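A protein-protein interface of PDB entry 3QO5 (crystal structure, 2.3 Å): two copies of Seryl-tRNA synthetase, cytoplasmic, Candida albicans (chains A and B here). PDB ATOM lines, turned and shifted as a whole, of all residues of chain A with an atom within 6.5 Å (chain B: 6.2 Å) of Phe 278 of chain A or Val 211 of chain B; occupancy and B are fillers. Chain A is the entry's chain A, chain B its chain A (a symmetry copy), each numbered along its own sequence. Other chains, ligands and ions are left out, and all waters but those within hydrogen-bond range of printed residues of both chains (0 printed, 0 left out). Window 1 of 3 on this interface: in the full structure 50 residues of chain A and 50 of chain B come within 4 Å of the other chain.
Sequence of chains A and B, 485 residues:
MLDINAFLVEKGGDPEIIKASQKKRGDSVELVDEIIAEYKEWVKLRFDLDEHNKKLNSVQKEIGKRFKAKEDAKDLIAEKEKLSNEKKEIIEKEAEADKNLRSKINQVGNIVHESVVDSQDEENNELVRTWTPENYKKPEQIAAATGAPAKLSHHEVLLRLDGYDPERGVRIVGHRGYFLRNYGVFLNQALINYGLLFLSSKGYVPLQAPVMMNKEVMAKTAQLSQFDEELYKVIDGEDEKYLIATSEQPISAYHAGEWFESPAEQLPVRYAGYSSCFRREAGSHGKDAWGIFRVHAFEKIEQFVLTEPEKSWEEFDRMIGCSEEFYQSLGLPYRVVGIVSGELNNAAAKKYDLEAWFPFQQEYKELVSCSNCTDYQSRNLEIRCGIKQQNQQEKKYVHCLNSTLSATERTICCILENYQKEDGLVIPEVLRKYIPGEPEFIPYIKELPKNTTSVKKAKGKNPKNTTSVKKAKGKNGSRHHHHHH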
ATOM      1  N   VAL A 173       6.235   2.975  25.150  1.00  0.00           N
ATOM      2  CA  VAL A 173       5.350   2.112  24.351  1.00  0.00           C
ATOM      3  C   VAL A 173       3.908   2.032  24.831  1.00  0.00           C
ATOM      4  O   VAL A 173       3.060   1.435  24.170  1.00  0.00           O
ATOM      5  CB  VAL A 173       5.933   0.674  24.215  1.00  0.00           C
ATOM      6  CG1 VAL A 173       6.073   0.038  25.547  1.00  0.00           C
ATOM      7  CG2 VAL A 173       5.055  -0.189  23.314  1.00  0.00           C
ATOM      8  N   VAL A 211       8.341 -14.280  14.513  1.00  0.00           N
ATOM      9  CA  VAL A 211       7.219 -13.719  15.241  1.00  0.00           C
ATOM     10  C   VAL A 211       6.205 -13.022  14.335  1.00  0.00           C
ATOM     11  O   VAL A 211       5.204 -12.487  14.813  1.00  0.00           O
ATOM     12  CB  VAL A 211       7.689 -12.716  16.304  1.00  0.00           C
ATOM     13  CG1 VAL A 211       8.523 -13.422  17.336  1.00  0.00           C
ATOM     14  CG2 VAL A 211       8.448 -11.515  15.650  1.00  0.00           C
ATOM     15  N   GLU A 230      -7.005 -10.525  19.559  1.00  0.00           N
ATOM     16  CA  GLU A 230      -5.793 -10.952  20.241  1.00  0.00           C
ATOM     17  C   GLU A 230      -4.533 -10.522  19.500  1.00  0.00           C
ATOM     18  O   GLU A 230      -3.531 -10.175  20.133  1.00  0.00           O
ATOM     19  CB  GLU A 230      -5.774 -12.465  20.493  1.00  0.00           C
ATOM     20  CG  GLU A 230      -4.917 -12.880  21.703  1.00  0.00           C
ATOM     21  CD  GLU A 230      -5.355 -12.194  23.009  1.00  0.00           C
ATOM     22  OE1 GLU A 230      -4.734 -11.171  23.381  1.00  0.00           O
ATOM     23  OE2 GLU A 230      -6.314 -12.675  23.664  1.00  0.00           O
ATOM     24  N   LEU A 231      -4.575 -10.516  18.169  1.00  0.00           N
ATOM     25  CA  LEU A 231      -3.341 -10.339  17.403  1.00  0.00           C
ATOM     26  C   LEU A 231      -3.130  -8.924  16.886  1.00  0.00           C
ATOM     27  O   LEU A 231      -4.050  -8.292  16.369  1.00  0.00           O
ATOM     28  CB  LEU A 231      -3.313 -11.315  16.218  1.00  0.00           C
ATOM     29  CG  LEU A 231      -3.545 -12.806  16.475  1.00  0.00           C
ATOM     30  CD1 LEU A 231      -3.661 -13.610  15.183  1.00  0.00           C
ATOM     31  CD2 LEU A 231      -2.489 -13.367  17.403  1.00  0.00           C
ATOM     32  N   TYR A 232      -1.885  -8.465  16.984  1.00  0.00           N
ATOM     33  CA  TYR A 232      -1.470  -7.215  16.363  1.00  0.00           C
ATOM     34  C   TYR A 232      -1.310  -7.459  14.874  1.00  0.00           C
ATOM     35  O   TYR A 232      -0.778  -8.485  14.455  1.00  0.00           O
ATOM     36  CB  TYR A 232      -0.123  -6.767  16.920  1.00  0.00           C
ATOM     37  CG  TYR A 232      -0.145  -6.275  18.339  1.00  0.00           C
ATOM     38  CD1 TYR A 232      -0.401  -4.934  18.626  1.00  0.00           C
ATOM     39  CD2 TYR A 232       0.042  -7.153  19.402  1.00  0.00           C
ATOM     40  CE1 TYR A 232      -0.431  -4.467  19.932  1.00  0.00           C
ATOM     41  CE2 TYR A 232       0.001  -6.704  20.714  1.00  0.00           C
ATOM     42  CZ  TYR A 232      -0.234  -5.357  20.973  1.00  0.00           C
ATOM     43  OH  TYR A 232      -0.268  -4.910  22.272  1.00  0.00           O
ATOM     44  N   LEU A 243       1.528 -10.388  14.107  1.00  0.00           N
ATOM     45  CA  LEU A 243       2.487 -10.829  15.105  1.00  0.00           C
ATOM     46  C   LEU A 243       1.877 -12.031  15.805  1.00  0.00           C
ATOM     47  O   LEU A 243       0.683 -12.032  16.079  1.00  0.00           O
ATOM     48  CB  LEU A 243       2.776  -9.726  16.118  1.00  0.00           C
ATOM     49  CG  LEU A 243       3.656  -8.598  15.575  1.00  0.00           C
ATOM     50  CD1 LEU A 243       3.758  -7.501  16.632  1.00  0.00           C
ATOM     51  CD2 LEU A 243       5.019  -9.111  15.220  1.00  0.00           C
ATOM     52  N   ILE A 244       2.687 -13.026  16.143  1.00  0.00           N
ATOM     53  CA  ILE A 244       2.154 -14.241  16.756  1.00  0.00           C
ATOM     54  C   ILE A 244       1.851 -14.018  18.254  1.00  0.00           C
ATOM     55  O   ILE A 244       2.487 -13.180  18.908  1.00  0.00           O
ATOM     56  CB  ILE A 244       3.119 -15.443  16.571  1.00  0.00           C
ATOM     57  CG1 ILE A 244       4.402 -15.225  17.380  1.00  0.00           C
ATOM     58  CG2 ILE A 244       3.514 -15.666  15.069  1.00  0.00           C
ATOM     59  CD1 ILE A 244       5.368 -16.444  17.414  1.00  0.00           C
ATOM     60  N   ALA A 245       0.859 -14.749  18.778  1.00  0.00           N
ATOM     61  CA  ALA A 245       0.540 -14.722  20.214  1.00  0.00           C
ATOM     62  C   ALA A 245       1.362 -15.782  20.929  1.00  0.00           C
ATOM     63  O   ALA A 245       1.461 -15.779  22.150  1.00  0.00           O
ATOM     64  CB  ALA A 245      -0.982 -14.973  20.467  1.00  0.00           C
ATOM     65  N   THR A 246       1.922 -16.715  20.159  1.00  0.00           N
ATOM     66  CA  THR A 246       2.643 -17.863  20.724  1.00  0.00           C
ATOM     67  C   THR A 246       3.321 -18.655  19.612  1.00  0.00           C
ATOM     68  O   THR A 246       2.814 -18.711  18.481  1.00  0.00           O
ATOM     69  CB  THR A 246       1.728 -18.844  21.516  1.00  0.00           C
ATOM     70  OG1 THR A 246       2.406 -20.082  21.737  1.00  0.00           O
ATOM     71  CG2 THR A 246       0.407 -19.111  20.775  1.00  0.00           C
ATOM     72  N   SER A 276       9.374 -14.661  21.209  1.00  0.00           N
ATOM     73  CA  SER A 276       8.565 -13.663  21.890  1.00  0.00           C
ATOM     74  C   SER A 276       7.089 -13.828  21.447  1.00  0.00           C
ATOM     75  O   SER A 276       6.798 -14.478  20.421  1.00  0.00           O
ATOM     76  CB  SER A 276       9.068 -12.260  21.577  1.00  0.00           C
ATOM     77  OG  SER A 276      10.306 -12.029  22.219  1.00  0.00           O
ATOM     78  N   CYS A 277       6.171 -13.246  22.224  1.00  0.00           N
ATOM     79  CA  CYS A 277       4.735 -13.417  22.017  1.00  0.00           C
ATOM     80  C   CYS A 277       4.080 -12.049  22.217  1.00  0.00           C
ATOM     81  O   CYS A 277       4.481 -11.267  23.090  1.00  0.00           O
ATOM     82  CB  CYS A 277       4.167 -14.396  23.062  1.00  0.00           C
ATOM     83  SG  CYS A 277       4.947 -16.061  22.993  1.00  0.00           S
ATOM     84  N   PHE A 278       3.035 -11.791  21.440  1.00  0.00           N
ATOM     85  CA  PHE A 278       2.395 -10.493  21.458  1.00  0.00           C
ATOM     86  C   PHE A 278       0.896 -10.658  21.541  1.00  0.00           C
ATOM     87  O   PHE A 278       0.297 -11.403  20.762  1.00  0.00           O
ATOM     88  CB  PHE A 278       2.805  -9.716  20.181  1.00  0.00           C
ATOM     89  CG  PHE A 278       4.300  -9.598  20.007  1.00  0.00           C
ATOM     90  CD1 PHE A 278       4.990  -8.522  20.544  1.00  0.00           C
ATOM     91  CD2 PHE A 278       5.022 -10.605  19.379  1.00  0.00           C
ATOM     92  CE1 PHE A 278       6.355  -8.434  20.422  1.00  0.00           C
ATOM     93  CE2 PHE A 278       6.402 -10.516  19.249  1.00  0.00           C
ATOM     94  CZ  PHE A 278       7.068  -9.427  19.772  1.00  0.00           C
ATOM     95  N   ARG A 279       0.307 -10.008  22.536  1.00  0.00           N
ATOM     96  CA  ARG A 279      -1.136 -10.110  22.753  1.00  0.00           C
ATOM     97  C   ARG A 279      -1.732  -8.718  22.944  1.00  0.00           C
ATOM     98  O   ARG A 279      -1.338  -7.986  23.869  1.00  0.00           O
ATOM     99  CB  ARG A 279      -1.348 -10.991  23.968  1.00  0.00           C
ATOM    100  CG  ARG A 279      -0.877 -12.434  23.683  1.00  0.00           C
ATOM    101  CD  ARG A 279      -1.273 -13.400  24.783  1.00  0.00           C
ATOM    102  NE  ARG A 279      -2.700 -13.331  25.044  1.00  0.00           N
ATOM    103  CZ  ARG A 279      -3.287 -13.869  26.103  1.00  0.00           C
ATOM    104  NH1 ARG A 279      -4.597 -13.744  26.265  1.00  0.00           N
ATOM    105  NH2 ARG A 279      -2.557 -14.515  27.004  1.00  0.00           N
ATOM    106  N   ARG A 280      -2.722  -8.369  22.128  1.00  0.00           N
ATOM    107  CA  ARG A 280      -3.407  -7.087  22.276  1.00  0.00           C
ATOM    108  C   ARG A 280      -4.186  -6.972  23.578  1.00  0.00           C
ATOM    109  O   ARG A 280      -4.362  -5.875  24.100  1.00  0.00           O
ATOM    110  CB  ARG A 280      -4.355  -6.883  21.094  1.00  0.00           C
ATOM    111  CG  ARG A 280      -3.670  -6.623  19.772  1.00  0.00           C
ATOM    112  CD  ARG A 280      -4.687  -6.280  18.696  1.00  0.00           C
ATOM    113  NE  ARG A 280      -5.544  -5.180  19.105  1.00  0.00           N
ATOM    114  CZ  ARG A 280      -6.821  -5.089  18.763  1.00  0.00           C
ATOM    115  NH1 ARG A 280      -7.371  -6.057  18.036  1.00  0.00           N
ATOM    116  NH2 ARG A 280      -7.548  -4.059  19.174  1.00  0.00           N
ATOM    117  N   VAL A 295       1.201  -8.982  30.313  1.00  0.00           N
ATOM    118  CA  VAL A 295       1.727  -7.860  29.536  1.00  0.00           C
ATOM    119  C   VAL A 295       1.522  -8.137  28.037  1.00  0.00           C
ATOM    120  O   VAL A 295       1.091  -9.216  27.649  1.00  0.00           O
ATOM    121  CB  VAL A 295       3.218  -7.626  29.834  1.00  0.00           C
ATOM    122  CG1 VAL A 295       3.354  -7.067  31.252  1.00  0.00           C
ATOM    123  CG2 VAL A 295       4.003  -8.908  29.729  1.00  0.00           C
ATOM    124  N   HIS A 296       1.803  -7.164  27.184  1.00  0.00           N
ATOM    125  CA  HIS A 296       1.509  -7.336  25.769  1.00  0.00           C
ATOM    126  C   HIS A 296       2.586  -8.106  25.021  1.00  0.00           C
ATOM    127  O   HIS A 296       2.342  -8.622  23.940  1.00  0.00           O
ATOM    128  CB  HIS A 296       1.305  -5.969  25.120  1.00  0.00           C
ATOM    129  CG  HIS A 296       0.077  -5.264  25.612  1.00  0.00           C
ATOM    130  ND1 HIS A 296      -1.194  -5.663  25.257  1.00  0.00           N
ATOM    131  CD2 HIS A 296      -0.078  -4.165  26.391  1.00  0.00           C
ATOM    132  CE1 HIS A 296      -2.079  -4.866  25.827  1.00  0.00           C
ATOM    133  NE2 HIS A 296      -1.426  -3.945  26.511  1.00  0.00           N
ATOM    134  N   ALA A 297       3.789  -8.131  25.566  1.00  0.00           N
ATOM    135  CA  ALA A 297       4.917  -8.762  24.895  1.00  0.00           C
ATOM    136  C   ALA A 297       5.741  -9.508  25.919  1.00  0.00           C
ATOM    137  O   ALA A 297       6.031  -8.947  26.969  1.00  0.00           O
ATOM    138  CB  ALA A 297       5.773  -7.733  24.153  1.00  0.00           C
ATOM    139  N   PHE A 298       6.082 -10.768  25.648  1.00  0.00           N
ATOM    140  CA  PHE A 298       6.799 -11.561  26.626  1.00  0.00           C
ATOM    141  C   PHE A 298       7.380 -12.734  25.888  1.00  0.00           C
ATOM    142  O   PHE A 298       7.027 -12.981  24.743  1.00  0.00           O
ATOM    143  CB  PHE A 298       5.865 -12.045  27.771  1.00  0.00           C
ATOM    144  CG  PHE A 298       4.672 -12.808  27.295  1.00  0.00           C
ATOM    145  CD1 PHE A 298       4.762 -14.171  27.093  1.00  0.00           C
ATOM    146  CD2 PHE A 298       3.498 -12.159  26.957  1.00  0.00           C
ATOM    147  CE1 PHE A 298       3.665 -14.906  26.641  1.00  0.00           C
ATOM    148  CE2 PHE A 298       2.397 -12.869  26.500  1.00  0.00           C
ATOM    149  CZ  PHE A 298       2.485 -14.253  26.325  1.00  0.00           C
ATOM    150  N   GLU A 299       8.244 -13.492  26.548  1.00  0.00           N
ATOM    151  CA  GLU A 299       8.831 -14.655  25.896  1.00  0.00           C
ATOM    152  C   GLU A 299       8.221 -15.937  26.430  1.00  0.00           C
ATOM    153  O   GLU A 299       7.702 -15.986  27.537  1.00  0.00           O
ATOM    154  CB  GLU A 299      10.347 -14.680  26.072  1.00  0.00           C
ATOM    155  CG  GLU A 299      11.061 -13.640  25.239  1.00  0.00           C
ATOM    156  CD  GLU A 299      10.797 -12.246  25.721  1.00  0.00           C
ATOM    157  OE1 GLU A 299      11.173 -11.912  26.877  1.00  0.00           O
ATOM    158  OE2 GLU A 299      10.171 -11.499  24.943  1.00  0.00           O
ATOM    159  N   ALA B 209      14.971  -4.018  25.882  1.00  0.00           N
ATOM    160  CA  ALA B 209      14.016  -3.008  25.467  1.00  0.00           C
ATOM    161  C   ALA B 209      12.760  -3.627  24.863  1.00  0.00           C
ATOM    162  O   ALA B 209      12.794  -4.732  24.323  1.00  0.00           O
ATOM    163  CB  ALA B 209      14.666  -2.068  24.468  1.00  0.00           C
ATOM    164  N   PRO B 210      11.631  -2.939  25.006  1.00  0.00           N
ATOM    165  CA  PRO B 210      10.401  -3.327  24.320  1.00  0.00           C
ATOM    166  C   PRO B 210      10.621  -3.134  22.839  1.00  0.00           C
ATOM    167  O   PRO B 210      11.384  -2.245  22.487  1.00  0.00           O
ATOM    168  CB  PRO B 210       9.364  -2.314  24.819  1.00  0.00           C
ATOM    169  CG  PRO B 210      10.151  -1.173  25.341  1.00  0.00           C
ATOM    170  CD  PRO B 210      11.457  -1.732  25.826  1.00  0.00           C
ATOM    171  N   VAL B 211       9.982  -3.936  21.994  1.00  0.00           N
ATOM    172  CA  VAL B 211      10.188  -3.843  20.562  1.00  0.00           C
ATOM    173  C   VAL B 211       9.100  -3.037  19.851  1.00  0.00           C
ATOM    174  O   VAL B 211       9.135  -2.882  18.630  1.00  0.00           O
ATOM    175  CB  VAL B 211      10.260  -5.234  19.916  1.00  0.00           C
ATOM    176  CG1 VAL B 211      11.454  -5.978  20.444  1.00  0.00           C
ATOM    177  CG2 VAL B 211       8.928  -6.025  20.128  1.00  0.00           C
ATOM    178  N   MET B 212       8.147  -2.516  20.608  1.00  0.00           N
ATOM    179  CA  MET B 212       7.176  -1.568  20.058  1.00  0.00           C
ATOM    180  C   MET B 212       7.409  -0.206  20.640  1.00  0.00           C
ATOM    181  O   MET B 212       7.793  -0.078  21.797  1.00  0.00           O
ATOM    182  CB  MET B 212       5.743  -1.978  20.376  1.00  0.00           C
ATOM    183  CG  MET B 212       5.322  -3.234  19.670  1.00  0.00           C
ATOM    184  SD  MET B 212       3.594  -3.623  19.917  1.00  0.00           S
ATOM    185  CE  MET B 212       3.512  -5.228  19.146  1.00  0.00           C
ATOM    186  N   MET B 213       7.157   0.816  19.841  1.00  0.00           N
ATOM    187  CA  MET B 213       7.319   2.184  20.300  1.00  0.00           C
ATOM    188  C   MET B 213       6.166   3.020  19.798  1.00  0.00           C
ATOM    189  O   MET B 213       5.703   2.842  18.675  1.00  0.00           O
ATOM    190  CB  MET B 213       8.614   2.790  19.768  1.00  0.00           C
ATOM    191  CG  MET B 213       9.741   2.887  20.784  1.00  0.00           C
ATOM    192  SD  MET B 213      11.254   3.649  20.113  1.00  0.00           S
ATOM    193  CE  MET B 213      11.174   5.330  20.762  1.00  0.00           C
ATOM    194  N   TYR B 242       5.167   1.537  16.213  1.00  0.00           N
ATOM    195  CA  TYR B 242       6.167   1.009  15.290  1.00  0.00           C
ATOM    196  C   TYR B 242       6.904  -0.142  15.948  1.00  0.00           C
ATOM    197  O   TYR B 242       7.076  -0.161  17.167  1.00  0.00           O
ATOM    198  CB  TYR B 242       7.185   2.097  14.950  1.00  0.00           C
ATOM    199  CG  TYR B 242       6.613   3.157  14.055  1.00  0.00           C
ATOM    200  CD1 TYR B 242       6.411   2.915  12.709  1.00  0.00           C
ATOM    201  CD2 TYR B 242       6.233   4.390  14.567  1.00  0.00           C
ATOM    202  CE1 TYR B 242       5.873   3.876  11.884  1.00  0.00           C
ATOM    203  CE2 TYR B 242       5.686   5.358  13.749  1.00  0.00           C
ATOM    204  CZ  TYR B 242       5.506   5.094  12.405  1.00  0.00           C
ATOM    205  OH  TYR B 242       4.972   6.050  11.569  1.00  0.00           O
ATOM    206  N   LEU B 243       7.372  -1.091  15.151  1.00  0.00           N
ATOM    207  CA  LEU B 243       8.354  -2.039  15.647  1.00  0.00           C
ATOM    208  C   LEU B 243       9.713  -1.372  15.523  1.00  0.00           C
ATOM    209  O   LEU B 243       9.973  -0.704  14.531  1.00  0.00           O
ATOM    210  CB  LEU B 243       8.331  -3.331  14.839  1.00  0.00           C
ATOM    211  CG  LEU B 243       7.124  -4.226  15.130  1.00  0.00           C
ATOM    212  CD1 LEU B 243       7.146  -5.412  14.169  1.00  0.00           C
ATOM    213  CD2 LEU B 243       7.146  -4.703  16.551  1.00  0.00           C
ATOM    214  N   ILE B 244      10.597  -1.589  16.489  1.00  0.00           N
ATOM    215  CA  ILE B 244      11.899  -0.922  16.466  1.00  0.00           C
ATOM    216  C   ILE B 244      12.858  -1.614  15.473  1.00  0.00           C
ATOM    217  O   ILE B 244      12.735  -2.820  15.213  1.00  0.00           O
ATOM    218  CB  ILE B 244      12.533  -0.865  17.882  1.00  0.00           C
ATOM    219  CG1 ILE B 244      12.915  -2.272  18.352  1.00  0.00           C
ATOM    220  CG2 ILE B 244      11.567  -0.232  18.944  1.00  0.00           C
ATOM    221  CD1 ILE B 244      13.721  -2.320  19.681  1.00  0.00           C
ATOM    222  N   PRO B 250      14.492   2.743  21.399  1.00  0.00           N
ATOM    223  CA  PRO B 250      13.871   2.978  22.714  1.00  0.00           C
ATOM    224  C   PRO B 250      14.869   3.360  23.821  1.00  0.00           C
ATOM    225  O   PRO B 250      14.563   4.176  24.679  1.00  0.00           O
ATOM    226  CB  PRO B 250      13.161   1.623  23.033  1.00  0.00           C
ATOM    227  CG  PRO B 250      13.957   0.573  22.207  1.00  0.00           C
ATOM    228  CD  PRO B 250      14.321   1.349  20.934  1.00  0.00           C
ATOM    229  N   SER B 275      17.534  -6.642  22.308  1.00  0.00           N
ATOM    230  CA  SER B 275      16.180  -6.779  21.810  1.00  0.00           C
ATOM    231  C   SER B 275      16.240  -7.470  20.477  1.00  0.00           C
ATOM    232  O   SER B 275      17.295  -7.537  19.867  1.00  0.00           O
ATOM    233  CB  SER B 275      15.532  -5.413  21.613  1.00  0.00           C
ATOM    234  OG  SER B 275      16.065  -4.711  20.501  1.00  0.00           O
ATOM    235  N   SER B 276      15.090  -7.945  20.020  1.00  0.00           N
ATOM    236  CA  SER B 276      14.948  -8.264  18.609  1.00  0.00           C
ATOM    237  C   SER B 276      14.809  -6.943  17.809  1.00  0.00           C
ATOM    238  O   SER B 276      14.515  -5.876  18.385  1.00  0.00           O
ATOM    239  CB  SER B 276      13.741  -9.163  18.380  1.00  0.00           C
ATOM    240  OG  SER B 276      13.993 -10.459  18.884  1.00  0.00           O
ATOM    241  N   CYS B 277      15.026  -7.025  16.494  1.00  0.00           N
ATOM    242  CA  CYS B 277      15.062  -5.853  15.622  1.00  0.00           C
ATOM    243  C   CYS B 277      14.309  -6.214  14.341  1.00  0.00           C
ATOM    244  O   CYS B 277      14.397  -7.346  13.843  1.00  0.00           O
ATOM    245  CB  CYS B 277      16.519  -5.510  15.262  1.00  0.00           C
ATOM    246  SG  CYS B 277      17.563  -5.148  16.734  1.00  0.00           S
ATOM    247  N   PHE B 278      13.616  -5.231  13.780  1.00  0.00           N
ATOM    248  CA  PHE B 278      12.778  -5.472  12.626  1.00  0.00           C
ATOM    249  C   PHE B 278      13.025  -4.411  11.579  1.00  0.00           C
ATOM    250  O   PHE B 278      12.990  -3.213  11.871  1.00  0.00           O
ATOM    251  CB  PHE B 278      11.296  -5.481  13.079  1.00  0.00           C
ATOM    252  CG  PHE B 278      11.015  -6.468  14.186  1.00  0.00           C
ATOM    253  CD1 PHE B 278      10.642  -7.771  13.893  1.00  0.00           C
ATOM    254  CD2 PHE B 278      11.204  -6.113  15.515  1.00  0.00           C
ATOM    255  CE1 PHE B 278      10.426  -8.681  14.899  1.00  0.00           C
ATOM    256  CE2 PHE B 278      10.982  -7.029  16.536  1.00  0.00           C
ATOM    257  CZ  PHE B 278      10.591  -8.315  16.224  1.00  0.00           C
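Val 211 of chain A touches Phe 278 of chain B, and with the chains exchanged Phe 278 of chain A touches Val 211 of chain B.
6 positions are printed for both chains.
The backbone carbonyl oxygen (O) of Ile 244 of chain A lies within hydrogen-bond range of the backbone NH (N) of Phe 278 of chain A (2.9 Å).
The backbone carbonyl oxygen (O) of Val 211 of chain B is in hydrogen-bond range of the backbone NH (N) of Ile 244 of chain B.
The backbone carbonyl oxygen (O) of Tyr 232 of chain A is in hydrogen-bond range of the backbone NH (N) of Leu 243 of chain A (3.0 Å).
The backbone NH (N) of Ile 244 of chain A lies within hydrogen-bond range of the backbone carbonyl oxygen (O) of Val 211 of chain A (2.9 Å).
The backbone NH (N) of Phe 278 of chain B sits at hydrogen-bond distance from the backbone carbonyl oxygen (O) of Ile 244 of chain B, 2.9 Å away.
OH of Tyr 232 of chain A sits at hydrogen-bond distance from ND1 of His 296 of chain A, 3.2 Å away.
Among the printed residues, pairs that only touch across the chains: Val 173 of chain A with Met 212 of chain B (3.1 Å), Val 211 of chain A with Phe 278 of chain B (3.5 Å), Tyr 232 of chain A with Met 212 of chain B (3.9 Å), Leu 243 of chain A with Met 212 of chain B (3.4 Å), Phe 278 of chain A with Val 211 of chain B (3.5 Å) and Phe 278 of chain A with Met 212 of chain B (3.9 Å).
Val 211 of chain B touches just one residue of chain A: Phe 278.
Printed residues of chain A within 4 Å of Met 212 of chain B: Val 173 (3.1 Å), Tyr 232 (3.9 Å), Leu 243 (3.4 Å) and Phe 278 (3.9 Å).
Of the printed residues of chain B, Val 211 of chain A touches Phe 278.
Printed residues of chain A within 4 Å of Phe 278 of chain B: Val 211 (3.5 Å).
Of the printed residues of chain B, Leu 243 of chain A touches Met 212 (3.4 Å).
The nearest residue of chain B that does not touch Phe 278 of chain A is Phe 278 of chain B (5.1 Å).
The nearest residue of chain A that does not touch Val 211 of chain B is Ala 297 of chain A (5.4 Å).
Hydrophobic or aromatic side chains of chain A that line the printed part of chain B: Val 173, Val 211, Tyr 232, Leu 243 and Phe 278.
Of the 13 printed residues of chain B, 3 touch a printed residue of chain A.
Printed residues of chain B that touch a printed residue of chain A: Val 211, Met 212 and Phe 278.
Hydrophobic or aromatic side chains of chain B within 4 Å of the printed part of chain A: Val 211, Met 212 and Phe 278.
Among the printed residues, 6 pairs touch across the chains.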
